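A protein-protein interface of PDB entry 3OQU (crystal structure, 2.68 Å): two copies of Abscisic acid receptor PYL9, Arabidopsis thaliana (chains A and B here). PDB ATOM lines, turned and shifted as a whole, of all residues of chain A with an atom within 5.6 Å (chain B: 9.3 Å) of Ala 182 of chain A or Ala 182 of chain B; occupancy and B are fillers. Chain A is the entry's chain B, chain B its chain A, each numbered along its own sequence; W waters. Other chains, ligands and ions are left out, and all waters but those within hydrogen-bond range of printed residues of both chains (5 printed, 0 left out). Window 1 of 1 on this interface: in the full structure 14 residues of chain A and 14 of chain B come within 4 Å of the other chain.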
ATOM      1  N   CYS A 177     -10.837  -7.920   4.627  1.00  0.00           N
ATOM      2  CA  CYS A 177     -12.052  -7.298   4.129  1.00  0.00           C
ATOM      3  C   CYS A 177     -12.645  -6.186   5.012  1.00  0.00           C
ATOM      4  O   CYS A 177     -13.167  -5.202   4.482  1.00  0.00           O
ATOM      5  CB  CYS A 177     -13.062  -8.338   3.620  1.00  0.00           C
ATOM      6  SG  CYS A 177     -12.804  -8.645   1.799  1.00  0.00           S
ATOM      7  N   TYR A 178     -12.513  -6.304   6.337  1.00  0.00           N
ATOM      8  CA  TYR A 178     -12.888  -5.195   7.219  1.00  0.00           C
ATOM      9  C   TYR A 178     -12.055  -3.928   6.974  1.00  0.00           C
ATOM     10  O   TYR A 178     -12.599  -2.826   6.939  1.00  0.00           O
ATOM     11  CB  TYR A 178     -12.844  -5.580   8.698  1.00  0.00           C
ATOM     12  CG  TYR A 178     -13.840  -6.640   9.097  1.00  0.00           C
ATOM     13  CD1 TYR A 178     -15.039  -6.801   8.401  1.00  0.00           C
ATOM     14  CD2 TYR A 178     -13.593  -7.476  10.188  1.00  0.00           C
ATOM     15  CE1 TYR A 178     -15.960  -7.775   8.770  1.00  0.00           C
ATOM     16  CE2 TYR A 178     -14.509  -8.457  10.565  1.00  0.00           C
ATOM     17  CZ  TYR A 178     -15.688  -8.595   9.851  1.00  0.00           C
ATOM     18  OH  TYR A 178     -16.591  -9.561  10.205  1.00  0.00           O
ATOM     19  N   PHE A 179     -10.749  -4.087   6.783  1.00  0.00           N
ATOM     20  CA  PHE A 179      -9.869  -2.946   6.529  1.00  0.00           C
ATOM     21  C   PHE A 179     -10.179  -2.264   5.187  1.00  0.00           C
ATOM     22  O   PHE A 179     -10.411  -1.052   5.134  1.00  0.00           O
ATOM     23  CB  PHE A 179      -8.399  -3.367   6.623  1.00  0.00           C
ATOM     24  CG  PHE A 179      -7.838  -3.340   8.035  1.00  0.00           C
ATOM     25  CD1 PHE A 179      -8.485  -4.001   9.084  1.00  0.00           C
ATOM     26  CD2 PHE A 179      -6.648  -2.667   8.307  1.00  0.00           C
ATOM     27  CE1 PHE A 179      -7.965  -3.982  10.370  1.00  0.00           C
ATOM     28  CE2 PHE A 179      -6.112  -2.644   9.599  1.00  0.00           C
ATOM     29  CZ  PHE A 179      -6.774  -3.302  10.631  1.00  0.00           C
ATOM     30  N   VAL A 180     -10.217  -3.038   4.110  1.00  0.00           N
ATOM     31  CA  VAL A 180     -10.554  -2.484   2.805  1.00  0.00           C
ATOM     32  C   VAL A 180     -11.929  -1.794   2.837  1.00  0.00           C
ATOM     33  O   VAL A 180     -12.098  -0.705   2.267  1.00  0.00           O
ATOM     34  CB  VAL A 180     -10.513  -3.551   1.687  1.00  0.00           C
ATOM     35  CG1 VAL A 180     -10.884  -2.930   0.348  1.00  0.00           C
ATOM     36  CG2 VAL A 180      -9.152  -4.181   1.610  1.00  0.00           C
ATOM     37  N   GLU A 181     -12.904  -2.410   3.508  1.00  0.00           N
ATOM     38  CA  GLU A 181     -14.240  -1.807   3.604  1.00  0.00           C
ATOM     39  C   GLU A 181     -14.204  -0.434   4.266  1.00  0.00           C
ATOM     40  O   GLU A 181     -14.977   0.449   3.900  1.00  0.00           O
ATOM     41  CB  GLU A 181     -15.191  -2.701   4.377  1.00  0.00           C
ATOM     42  CG  GLU A 181     -15.798  -3.832   3.587  1.00  0.00           C
ATOM     43  CD  GLU A 181     -16.499  -4.816   4.500  1.00  0.00           C
ATOM     44  OE1 GLU A 181     -16.979  -4.395   5.577  1.00  0.00           O
ATOM     45  OE2 GLU A 181     -16.561  -6.013   4.151  1.00  0.00           O
ATOM     46  N   ALA A 182     -13.309  -0.272   5.241  1.00  0.00           N
ATOM     47  CA  ALA A 182     -13.117   1.000   5.925  1.00  0.00           C
ATOM     48  C   ALA A 182     -12.682   2.071   4.922  1.00  0.00           C
ATOM     49  O   ALA A 182     -13.202   3.193   4.932  1.00  0.00           O
ATOM     50  CB  ALA A 182     -12.102   0.853   7.058  1.00  0.00           C
ATOM     51  N   LEU A 183     -11.752   1.709   4.040  1.00  0.00           N
ATOM     52  CA  LEU A 183     -11.293   2.616   2.993  1.00  0.00           C
ATOM     53  C   LEU A 183     -12.430   3.003   2.058  1.00  0.00           C
ATOM     54  O   LEU A 183     -12.617   4.181   1.727  1.00  0.00           O
ATOM     55  CB  LEU A 183     -10.154   1.988   2.199  1.00  0.00           C
ATOM     56  CG  LEU A 183      -8.858   1.785   2.988  1.00  0.00           C
ATOM     57  CD1 LEU A 183      -7.903   0.937   2.172  1.00  0.00           C
ATOM     58  CD2 LEU A 183      -8.224   3.129   3.401  1.00  0.00           C
ATOM     59  N   ILE A 184     -13.208   2.010   1.645  1.00  0.00           N
ATOM     60  CA  ILE A 184     -14.289   2.265   0.704  1.00  0.00           C
ATOM     61  C   ILE A 184     -15.408   3.108   1.331  1.00  0.00           C
ATOM     62  O   ILE A 184     -15.938   4.017   0.681  1.00  0.00           O
ATOM     63  CB  ILE A 184     -14.770   0.961   0.027  1.00  0.00           C
ATOM     64  CG1 ILE A 184     -13.627   0.440  -0.853  1.00  0.00           C
ATOM     65  CG2 ILE A 184     -16.036   1.217  -0.802  1.00  0.00           C
ATOM     66  CD1 ILE A 184     -13.844  -0.881  -1.492  1.00  0.00           C
ATOM     67  N   ARG A 185     -15.736   2.839   2.595  1.00  0.00           N
ATOM     68  CA  ARG A 185     -16.719   3.663   3.297  1.00  0.00           C
ATOM     69  C   ARG A 185     -16.270   5.129   3.309  1.00  0.00           C
ATOM     70  O   ARG A 185     -17.072   6.029   3.042  1.00  0.00           O
ATOM     71  CB  ARG A 185     -16.984   3.150   4.721  1.00  0.00           C
ATOM     72  CG  ARG A 185     -17.703   1.808   4.762  1.00  0.00           C
ATOM     73  CD  ARG A 185     -17.841   1.253   6.176  1.00  0.00           C
ATOM     74  NE  ARG A 185     -18.970   1.872   6.864  1.00  0.00           N
ATOM     75  CZ  ARG A 185     -19.100   1.957   8.186  1.00  0.00           C
ATOM     76  NH1 ARG A 185     -18.165   1.460   8.989  1.00  0.00           N
ATOM     77  NH2 ARG A 185     -20.170   2.551   8.704  1.00  0.00           N
ATOM     78  N   CYS A 186     -14.986   5.351   3.601  1.00  0.00           N
ATOM     79  CA  CYS A 186     -14.395   6.692   3.590  1.00  0.00           C
ATOM     80  C   CYS A 186     -14.647   7.370   2.246  1.00  0.00           C
ATOM     81  O   CYS A 186     -15.181   8.480   2.206  1.00  0.00           O
ATOM     82  CB  CYS A 186     -12.897   6.635   3.903  1.00  0.00           C
ATOM     83  SG  CYS A 186     -12.481   6.404   5.667  1.00  0.00           S
ATOM     84  N   ASN A 187     -14.303   6.676   1.159  1.00  0.00           N
ATOM     85  CA  ASN A 187     -14.528   7.157  -0.200  1.00  0.00           C
ATOM     86  C   ASN A 187     -15.993   7.494  -0.501  1.00  0.00           C
ATOM     87  O   ASN A 187     -16.284   8.606  -0.938  1.00  0.00           O
ATOM     88  CB  ASN A 187     -13.978   6.164  -1.240  1.00  0.00           C
ATOM     89  CG  ASN A 187     -12.446   6.053  -1.214  1.00  0.00           C
ATOM     90  OD1 ASN A 187     -11.758   6.800  -0.513  1.00  0.00           O
ATOM     91  ND2 ASN A 187     -11.908   5.105  -1.987  1.00  0.00           N
ATOM     92  N   SER B  54     -19.364   5.560  17.907  1.00  0.00           N
ATOM     93  CA  SER B  54     -20.112   4.545  17.184  1.00  0.00           C
ATOM     94  C   SER B  54     -20.279   3.280  18.009  1.00  0.00           C
ATOM     95  O   SER B  54     -19.585   3.083  18.996  1.00  0.00           O
ATOM     96  CB  SER B  54     -19.428   4.227  15.862  1.00  0.00           C
ATOM     97  OG  SER B  54     -20.268   3.417  15.068  1.00  0.00           O
ATOM     98  N   LEU B  56     -21.090  -1.133  17.728  1.00  0.00           N
ATOM     99  CA  LEU B  56     -21.128  -2.299  16.859  1.00  0.00           C
ATOM    100  C   LEU B  56     -21.828  -3.469  17.522  1.00  0.00           C
ATOM    101  O   LEU B  56     -21.678  -3.688  18.727  1.00  0.00           O
ATOM    102  CB  LEU B  56     -19.724  -2.674  16.384  1.00  0.00           C
ATOM    103  CG  LEU B  56     -19.127  -1.589  15.478  1.00  0.00           C
ATOM    104  CD1 LEU B  56     -18.070  -0.763  16.223  1.00  0.00           C
ATOM    105  CD2 LEU B  56     -18.546  -2.184  14.227  1.00  0.00           C
ATOM    106  N   PRO B  82      -7.286 -10.150  17.594  1.00  0.00           N
ATOM    107  CA  PRO B  82      -6.293 -10.710  16.672  1.00  0.00           C
ATOM    108  C   PRO B  82      -5.015  -9.879  16.489  1.00  0.00           C
ATOM    109  O   PRO B  82      -4.035 -10.382  15.930  1.00  0.00           O
ATOM    110  CB  PRO B  82      -7.059 -10.795  15.357  1.00  0.00           C
ATOM    111  CG  PRO B  82      -8.056  -9.697  15.443  1.00  0.00           C
ATOM    112  CD  PRO B  82      -8.463  -9.624  16.881  1.00  0.00           C
ATOM    113  N   PHE B  83      -5.017  -8.627  16.940  1.00  0.00           N
ATOM    114  CA  PHE B  83      -3.857  -7.760  16.715  1.00  0.00           C
ATOM    115  C   PHE B  83      -2.933  -7.610  17.932  1.00  0.00           C
ATOM    116  O   PHE B  83      -1.834  -7.067  17.819  1.00  0.00           O
ATOM    117  CB  PHE B  83      -4.290  -6.394  16.153  1.00  0.00           C
ATOM    118  CG  PHE B  83      -5.061  -6.492  14.861  1.00  0.00           C
ATOM    119  CD1 PHE B  83      -4.489  -7.076  13.734  1.00  0.00           C
ATOM    120  CD2 PHE B  83      -6.366  -6.007  14.774  1.00  0.00           C
ATOM    121  CE1 PHE B  83      -5.213  -7.177  12.540  1.00  0.00           C
ATOM    122  CE2 PHE B  83      -7.096  -6.102  13.586  1.00  0.00           C
ATOM    123  CZ  PHE B  83      -6.525  -6.684  12.472  1.00  0.00           C
ATOM    124  N   LEU B 107       0.645  -2.140  11.828  1.00  0.00           N
ATOM    125  CA  LEU B 107      -0.331  -1.156  12.288  1.00  0.00           C
ATOM    126  C   LEU B 107       0.382   0.157  12.619  1.00  0.00           C
ATOM    127  O   LEU B 107       1.598   0.144  12.841  1.00  0.00           O
ATOM    128  CB  LEU B 107      -1.092  -1.705  13.506  1.00  0.00           C
ATOM    129  CG  LEU B 107      -2.014  -2.870  13.123  1.00  0.00           C
ATOM    130  CD1 LEU B 107      -2.304  -3.776  14.285  1.00  0.00           C
ATOM    131  CD2 LEU B 107      -3.316  -2.362  12.522  1.00  0.00           C
ATOM    132  N   PHE B 163     -17.827   3.094  21.420  1.00  0.00           N
ATOM    133  CA  PHE B 163     -16.677   3.880  21.854  1.00  0.00           C
ATOM    134  C   PHE B 163     -16.853   5.378  21.596  1.00  0.00           C
ATOM    135  O   PHE B 163     -17.736   5.800  20.849  1.00  0.00           O
ATOM    136  CB  PHE B 163     -15.413   3.388  21.149  1.00  0.00           C
ATOM    137  CG  PHE B 163     -15.458   3.575  19.668  1.00  0.00           C
ATOM    138  CD1 PHE B 163     -14.944   4.731  19.083  1.00  0.00           C
ATOM    139  CD2 PHE B 163     -16.057   2.617  18.853  1.00  0.00           C
ATOM    140  CE1 PHE B 163     -15.008   4.922  17.704  1.00  0.00           C
ATOM    141  CE2 PHE B 163     -16.122   2.799  17.469  1.00  0.00           C
ATOM    142  CZ  PHE B 163     -15.596   3.953  16.897  1.00  0.00           C
ATOM    143  N   ASP B 174     -15.663  10.895  10.166  1.00  0.00           N
ATOM    144  CA  ASP B 174     -15.928   9.697   9.383  1.00  0.00           C
ATOM    145  C   ASP B 174     -14.701   8.802   9.287  1.00  0.00           C
ATOM    146  O   ASP B 174     -14.779   7.613   9.595  1.00  0.00           O
ATOM    147  CB  ASP B 174     -16.443  10.068   7.989  1.00  0.00           C
ATOM    148  CG  ASP B 174     -17.800  10.770   8.031  1.00  0.00           C
ATOM    149  OD1 ASP B 174     -18.661  10.401   8.866  1.00  0.00           O
ATOM    150  OD2 ASP B 174     -18.005  11.693   7.213  1.00  0.00           O
ATOM    151  N   GLU B 175     -13.571   9.376   8.882  1.00  0.00           N
ATOM    152  CA  GLU B 175     -12.325   8.623   8.762  1.00  0.00           C
ATOM    153  C   GLU B 175     -11.998   7.940  10.075  1.00  0.00           C
ATOM    154  O   GLU B 175     -11.780   6.727  10.119  1.00  0.00           O
ATOM    155  CB  GLU B 175     -11.166   9.532   8.337  1.00  0.00           C
ATOM    156  CG  GLU B 175     -11.185   9.907   6.862  1.00  0.00           C
ATOM    157  CD  GLU B 175     -10.481  11.226   6.552  1.00  0.00           C
ATOM    158  OE1 GLU B 175      -9.538  11.602   7.280  1.00  0.00           O
ATOM    159  OE2 GLU B 175     -10.877  11.883   5.567  1.00  0.00           O
ATOM    160  N   THR B 176     -11.997   8.725  11.147  1.00  0.00           N
ATOM    161  CA  THR B 176     -11.622   8.235  12.460  1.00  0.00           C
ATOM    162  C   THR B 176     -12.516   7.062  12.861  1.00  0.00           C
ATOM    163  O   THR B 176     -12.032   5.966  13.175  1.00  0.00           O
ATOM    164  CB  THR B 176     -11.689   9.362  13.488  1.00  0.00           C
ATOM    165  OG1 THR B 176     -10.782  10.401  13.097  1.00  0.00           O
ATOM    166  CG2 THR B 176     -11.331   8.859  14.887  1.00  0.00           C
ATOM    167  N   CYS B 177     -13.821   7.285  12.804  1.00  0.00           N
ATOM    168  CA  CYS B 177     -14.769   6.266  13.233  1.00  0.00           C
ATOM    169  C   CYS B 177     -14.842   5.041  12.315  1.00  0.00           C
ATOM    170  O   CYS B 177     -14.962   3.918  12.813  1.00  0.00           O
ATOM    171  CB  CYS B 177     -16.146   6.879  13.545  1.00  0.00           C
ATOM    172  SG  CYS B 177     -16.317   7.270  15.344  1.00  0.00           S
ATOM    173  N   TYR B 178     -14.735   5.237  10.999  1.00  0.00           N
ATOM    174  CA  TYR B 178     -14.662   4.085  10.094  1.00  0.00           C
ATOM    175  C   TYR B 178     -13.448   3.188  10.386  1.00  0.00           C
ATOM    176  O   TYR B 178     -13.555   1.965  10.320  1.00  0.00           O
ATOM    177  CB  TYR B 178     -14.667   4.481   8.613  1.00  0.00           C
ATOM    178  CG  TYR B 178     -15.941   5.123   8.109  1.00  0.00           C
ATOM    179  CD1 TYR B 178     -17.185   4.801   8.656  1.00  0.00           C
ATOM    180  CD2 TYR B 178     -15.899   6.040   7.059  1.00  0.00           C
ATOM    181  CE1 TYR B 178     -18.354   5.399   8.184  1.00  0.00           C
ATOM    182  CE2 TYR B 178     -17.053   6.639   6.578  1.00  0.00           C
ATOM    183  CZ  TYR B 178     -18.279   6.317   7.143  1.00  0.00           C
ATOM    184  OH  TYR B 178     -19.420   6.919   6.656  1.00  0.00           O
ATOM    185  N   PHE B 179     -12.305   3.790  10.710  1.00  0.00           N
ATOM    186  CA  PHE B 179     -11.100   3.015  11.014  1.00  0.00           C
ATOM    187  C   PHE B 179     -11.219   2.265  12.345  1.00  0.00           C
ATOM    188  O   PHE B 179     -10.992   1.055  12.404  1.00  0.00           O
ATOM    189  CB  PHE B 179      -9.847   3.900  10.991  1.00  0.00           C
ATOM    190  CG  PHE B 179      -9.234   4.074   9.615  1.00  0.00           C
ATOM    191  CD1 PHE B 179      -7.874   3.837   9.417  1.00  0.00           C
ATOM    192  CD2 PHE B 179     -10.009   4.477   8.521  1.00  0.00           C
ATOM    193  CE1 PHE B 179      -7.290   4.007   8.157  1.00  0.00           C
ATOM    194  CE2 PHE B 179      -9.441   4.644   7.266  1.00  0.00           C
ATOM    195  CZ  PHE B 179      -8.072   4.412   7.082  1.00  0.00           C
ATOM    196  N   VAL B 180     -11.594   2.969  13.407  1.00  0.00           N
ATOM    197  CA  VAL B 180     -11.778   2.321  14.704  1.00  0.00           C
ATOM    198  C   VAL B 180     -12.810   1.194  14.578  1.00  0.00           C
ATOM    199  O   VAL B 180     -12.606   0.102  15.140  1.00  0.00           O
ATOM    200  CB  VAL B 180     -12.163   3.326  15.818  1.00  0.00           C
ATOM    201  CG1 VAL B 180     -12.356   2.614  17.144  1.00  0.00           C
ATOM    202  CG2 VAL B 180     -11.099   4.392  15.961  1.00  0.00           C
ATOM    203  N   GLU B 181     -13.894   1.440  13.828  1.00  0.00           N
ATOM    204  CA  GLU B 181     -14.918   0.402  13.601  1.00  0.00           C
ATOM    205  C   GLU B 181     -14.342  -0.856  12.943  1.00  0.00           C
ATOM    206  O   GLU B 181     -14.808  -1.966  13.213  1.00  0.00           O
ATOM    207  CB  GLU B 181     -16.081   0.926  12.759  1.00  0.00           C
ATOM    208  CG  GLU B 181     -17.144   1.724  13.527  1.00  0.00           C
ATOM    209  CD  GLU B 181     -18.060   2.512  12.590  1.00  0.00           C
ATOM    210  OE1 GLU B 181     -18.196   2.138  11.401  1.00  0.00           O
ATOM    211  OE2 GLU B 181     -18.645   3.515  13.036  1.00  0.00           O
ATOM    212  N   ALA B 182     -13.336  -0.675  12.084  1.00  0.00           N
ATOM    213  CA  ALA B 182     -12.674  -1.797  11.428  1.00  0.00           C
ATOM    214  C   ALA B 182     -11.995  -2.687  12.468  1.00  0.00           C
ATOM    215  O   ALA B 182     -12.121  -3.913  12.432  1.00  0.00           O
ATOM    216  CB  ALA B 182     -11.681  -1.300  10.397  1.00  0.00           C
ATOM    217  N   LEU B 183     -11.311  -2.058  13.419  1.00  0.00           N
ATOM    218  CA  LEU B 183     -10.682  -2.772  14.524  1.00  0.00           C
ATOM    219  C   LEU B 183     -11.696  -3.524  15.377  1.00  0.00           C
ATOM    220  O   LEU B 183     -11.472  -4.688  15.751  1.00  0.00           O
ATOM    221  CB  LEU B 183      -9.878  -1.811  15.384  1.00  0.00           C
ATOM    222  CG  LEU B 183      -8.743  -1.147  14.606  1.00  0.00           C
ATOM    223  CD1 LEU B 183      -8.131  -0.023  15.424  1.00  0.00           C
ATOM    224  CD2 LEU B 183      -7.686  -2.171  14.161  1.00  0.00           C
ATOM    225  N   ILE B 184     -12.819  -2.880  15.677  1.00  0.00           N
ATOM    226  CA  ILE B 184     -13.803  -3.509  16.558  1.00  0.00           C
ATOM    227  C   ILE B 184     -14.521  -4.689  15.884  1.00  0.00           C
ATOM    228  O   ILE B 184     -14.755  -5.722  16.517  1.00  0.00           O
ATOM    229  CB  ILE B 184     -14.741  -2.470  17.204  1.00  0.00           C
ATOM    230  CG1 ILE B 184     -13.885  -1.495  18.019  1.00  0.00           C
ATOM    231  CG2 ILE B 184     -15.775  -3.150  18.089  1.00  0.00           C
ATOM    232  CD1 ILE B 184     -14.648  -0.474  18.836  1.00  0.00           C
ATOM    233  N   ARG B 185     -14.827  -4.560  14.596  1.00  0.00           N
ATOM    234  CA  ARG B 185     -15.397  -5.685  13.855  1.00  0.00           C
ATOM    235  C   ARG B 185     -14.430  -6.874  13.875  1.00  0.00           C
ATOM    236  O   ARG B 185     -14.852  -8.012  14.086  1.00  0.00           O
ATOM    237  CB  ARG B 185     -15.743  -5.285  12.417  1.00  0.00           C
ATOM    238  CG  ARG B 185     -16.782  -4.189  12.314  1.00  0.00           C
ATOM    239  CD  ARG B 185     -16.979  -3.723  10.881  1.00  0.00           C
ATOM    240  NE  ARG B 185     -17.876  -4.629  10.166  1.00  0.00           N
ATOM    241  CZ  ARG B 185     -17.924  -4.774   8.845  1.00  0.00           C
ATOM    242  NH1 ARG B 185     -17.121  -4.071   8.057  1.00  0.00           N
ATOM    243  NH2 ARG B 185     -18.779  -5.634   8.310  1.00  0.00           N
ATOM    244  N   CYS B 186     -13.139  -6.606  13.664  1.00  0.00           N
ATOM    245  CA  CYS B 186     -12.112  -7.643  13.738  1.00  0.00           C
ATOM    246  C   CYS B 186     -12.172  -8.361  15.083  1.00  0.00           C
ATOM    247  O   CYS B 186     -12.250  -9.583  15.124  1.00  0.00           O
ATOM    248  CB  CYS B 186     -10.721  -7.059  13.487  1.00  0.00           C
ATOM    249  SG  CYS B 186     -10.332  -6.701  11.745  1.00  0.00           S
ATOM    250  N   ASN B 187     -12.169  -7.593  16.171  1.00  0.00           N
ATOM    251  CA  ASN B 187     -12.239  -8.138  17.529  1.00  0.00           C
ATOM    252  C   ASN B 187     -13.512  -8.956  17.806  1.00  0.00           C
ATOM    253  O   ASN B 187     -13.428 -10.075  18.325  1.00  0.00           O
ATOM    254  CB  ASN B 187     -12.079  -7.020  18.579  1.00  0.00           C
ATOM    255  CG  ASN B 187     -10.689  -6.353  18.547  1.00  0.00           C
ATOM    256  OD1 ASN B 187      -9.724  -6.908  18.014  1.00  0.00           O
ATOM    257  ND2 ASN B 187     -10.593  -5.153  19.137  1.00  0.00           N
ATOM    258  N   LEU B 188     -14.678  -8.414  17.458  1.00  0.00           N
ATOM    259  CA  LEU B 188     -15.947  -9.091  17.725  1.00  0.00           C
ATOM    260  C   LEU B 188     -16.176 -10.332  16.848  1.00  0.00           C
ATOM    261  O   LEU B 188     -16.815 -11.305  17.277  1.00  0.00           O
ATOM    262  CB  LEU B 188     -17.125  -8.120  17.582  1.00  0.00           C
ATOM    263  CG  LEU B 188     -17.117  -6.860  18.458  1.00  0.00           C
ATOM    264  CD1 LEU B 188     -18.414  -6.078  18.259  1.00  0.00           C
ATOM    265  CD2 LEU B 188     -16.876  -7.172  19.947  1.00  0.00           C
ATOM    266  N   LYS B 189     -15.661 -10.291  15.622  1.00  0.00           N
ATOM    267  CA  LYS B 189     -15.747 -11.432  14.719  1.00  0.00           C
ATOM    268  C   LYS B 189     -14.869 -12.556  15.255  1.00  0.00           C
ATOM    269  O   LYS B 189     -15.252 -13.734  15.229  1.00  0.00           O
ATOM    270  CB  LYS B 189     -15.292 -11.047  13.309  1.00  0.00           C
ATOM    271  CG  LYS B 189     -16.115 -11.648  12.186  1.00  0.00           C
ATOM    272  CD  LYS B 189     -16.169 -13.157  12.209  1.00  0.00           C
ATOM    273  CE  LYS B 189     -16.944 -13.677  11.025  1.00  0.00           C
ATOM    274  NZ  LYS B 189     -16.444 -15.031  10.683  1.00  0.00           N
ATOM    275  N   SER B 190     -13.687 -12.184  15.735  1.00  0.00           N
ATOM    276  CA  SER B 190     -12.778 -13.155  16.315  1.00  0.00           C
ATOM    277  C   SER B 190     -13.392 -13.727  17.588  1.00  0.00           C
ATOM    278  O   SER B 190     -13.367 -14.947  17.800  1.00  0.00           O
ATOM    279  CB  SER B 190     -11.415 -12.534  16.586  1.00  0.00           C
ATOM    280  OG  SER B 190     -10.524 -13.525  17.051  1.00  0.00           O
HETATM  281  O   HOH W   1     -15.211  -2.280   8.400  1.00  0.00           O
HETATM  282  O   HOH W   2     -19.015  -1.770   6.549  1.00  0.00           O
HETATM  283  O   HOH W   3     -15.677   0.413   8.650  1.00  0.00           O
HETATM  284  O   HOH W   4     -18.860  -1.355  10.074  1.00  0.00           O
HETATM  285  O   HOH W   5     -20.794   3.624  11.210  1.00  0.00           O
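Of the printed residues of chain A, Ala 182 of chain B touches Tyr 178 and Ala 182.
Of the printed residues of chain B, Leu 183 of chain A touches Phe 179.
Of the printed residues of chain A, Phe 179 of chain B touches Leu 183 (3.9 Å) and Cys 186 (3.9 Å).
Printed residues of chain B within 4 Å of Phe 179 of chain A: Phe 83, Leu 183 and Cys 186.
Val 180 of chain B touches none of the printed residues of chain A.
Val 180 of chain A touches none of the printed residues of chain B.
The nearest printed residue of chain B that does not touch Ala 182 of chain A is Phe 179 of chain B (4.4 Å).
The nearest printed residue of chain A that does not touch Lys 189 of chain B is Cys 177 of chain A (9.7 Å).
Among the printed residues, merely in contact across the chains: Tyr 178 of chain A with Ala 182 of chain B (3.9 Å), Tyr 178 of chain A with Arg 185 of chain B (3.5 Å), Tyr 178 of chain A with Cys 186 of chain B (3.6 Å), Tyr 178 of chain A with Lys 189 of chain B (2.9 Å), Phe 179 of chain A with Phe 83 of chain B (3.7 Å), Phe 179 of chain A with Leu 183 of chain B (3.8 Å), Phe 179 of chain A with Cys 186 of chain B (3.9 Å), Ala 182 of chain A with Tyr 178 of chain B (3.7 Å), Ala 182 of chain A with Ala 182 of chain B (3.995 Å), Leu 183 of chain A with Phe 179 of chain B (3.9 Å), Arg 185 of chain A with Tyr 178 of chain B (3.4 Å), Cys 186 of chain A with Glu 175 of chain B (3.8 Å), Cys 186 of chain A with Tyr 178 of chain B (3.6 Å) and Cys 186 of chain A with Phe 179 of chain B (3.9 Å).
Water W1 lies within hydrogen-bond range of NH1 of Arg 185 of chain B (2.6 Å) and O of Tyr 178 of chain A (3.0 Å).
Water W3 lies within hydrogen-bond range of NH1 of Arg 185 of chain A (2.7 Å) and O of Tyr 178 of chain B (3.1 Å).
Water W5 bridges NH2 of Arg 185 of chain A and OE2 of Glu 181 of chain B.
Water W4 bridges the guanidinium group of Arg 185 of chain A (3.1 Å) and the guanidinium group of Arg 185 of chain B (3.4 Å).
Water W2 bridges NH1 of Arg 185 of chain B (3.3 Å) and OE1 of Glu 181 of chain A (3.5 Å).
The backbone carbonyl oxygen of Ala 182 of chain B sits at hydrogen-bond distance from the side-chain sulfur of Cys 186 of chain B (3.4 Å).
The side-chain carboxylate (OE2) of Glu 181 of chain B lies within hydrogen-bond range of the side-chain hydroxyl (OG) of Ser 54 of chain B, at 2.6 Å.
O of Ala 182 of chain A lies within hydrogen-bond range of SG of Cys 186 of chain A.
The side-chain carboxylate (OE1) of Glu 181 of chain A is in salt-bridge range of the guanidinium group (NH1) of Arg 185 of chain B (2.5 Å).
The side-chain carboxylate of Glu 181 of chain B lies within salt-bridge range of the guanidinium group of Arg 185 of chain A (2.5 Å).
Of the 11 printed residues of chain A, 7 touch a printed residue of chain B.
Hydrophobic or aromatic side chains of chain B that line the printed part of chain A: Phe 83, Tyr 178, Phe 179, Ala 182 and Leu 183.
Among the printed residues, 16 pairs touch across the chains.
Among the printed residues, Asp or Glu carboxylates within 4 Å of a Lys or Arg side-chain nitrogen of the other chain: Glu 181 of chain A with Arg 185 of chain B and Arg 185 of chain A with Glu 181 of chain B.
Tyr 178 of chain A touches Ala 182 of chain B, and with the chains exchanged Ala 182 of chain A touches Tyr 178 of chain B.
Tyr 178 of chain A touches Arg 185 of chain B, and with the chains exchanged Arg 185 of chain A touches Tyr 178 of chain B.
Phe 179 of chain A touches Cys 186 of chain B, and with the chains exchanged Cys 186 of chain A touches Phe 179 of chain B.
Ala 182 of chain B touches its own counterpart, Ala 182 of chain A.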
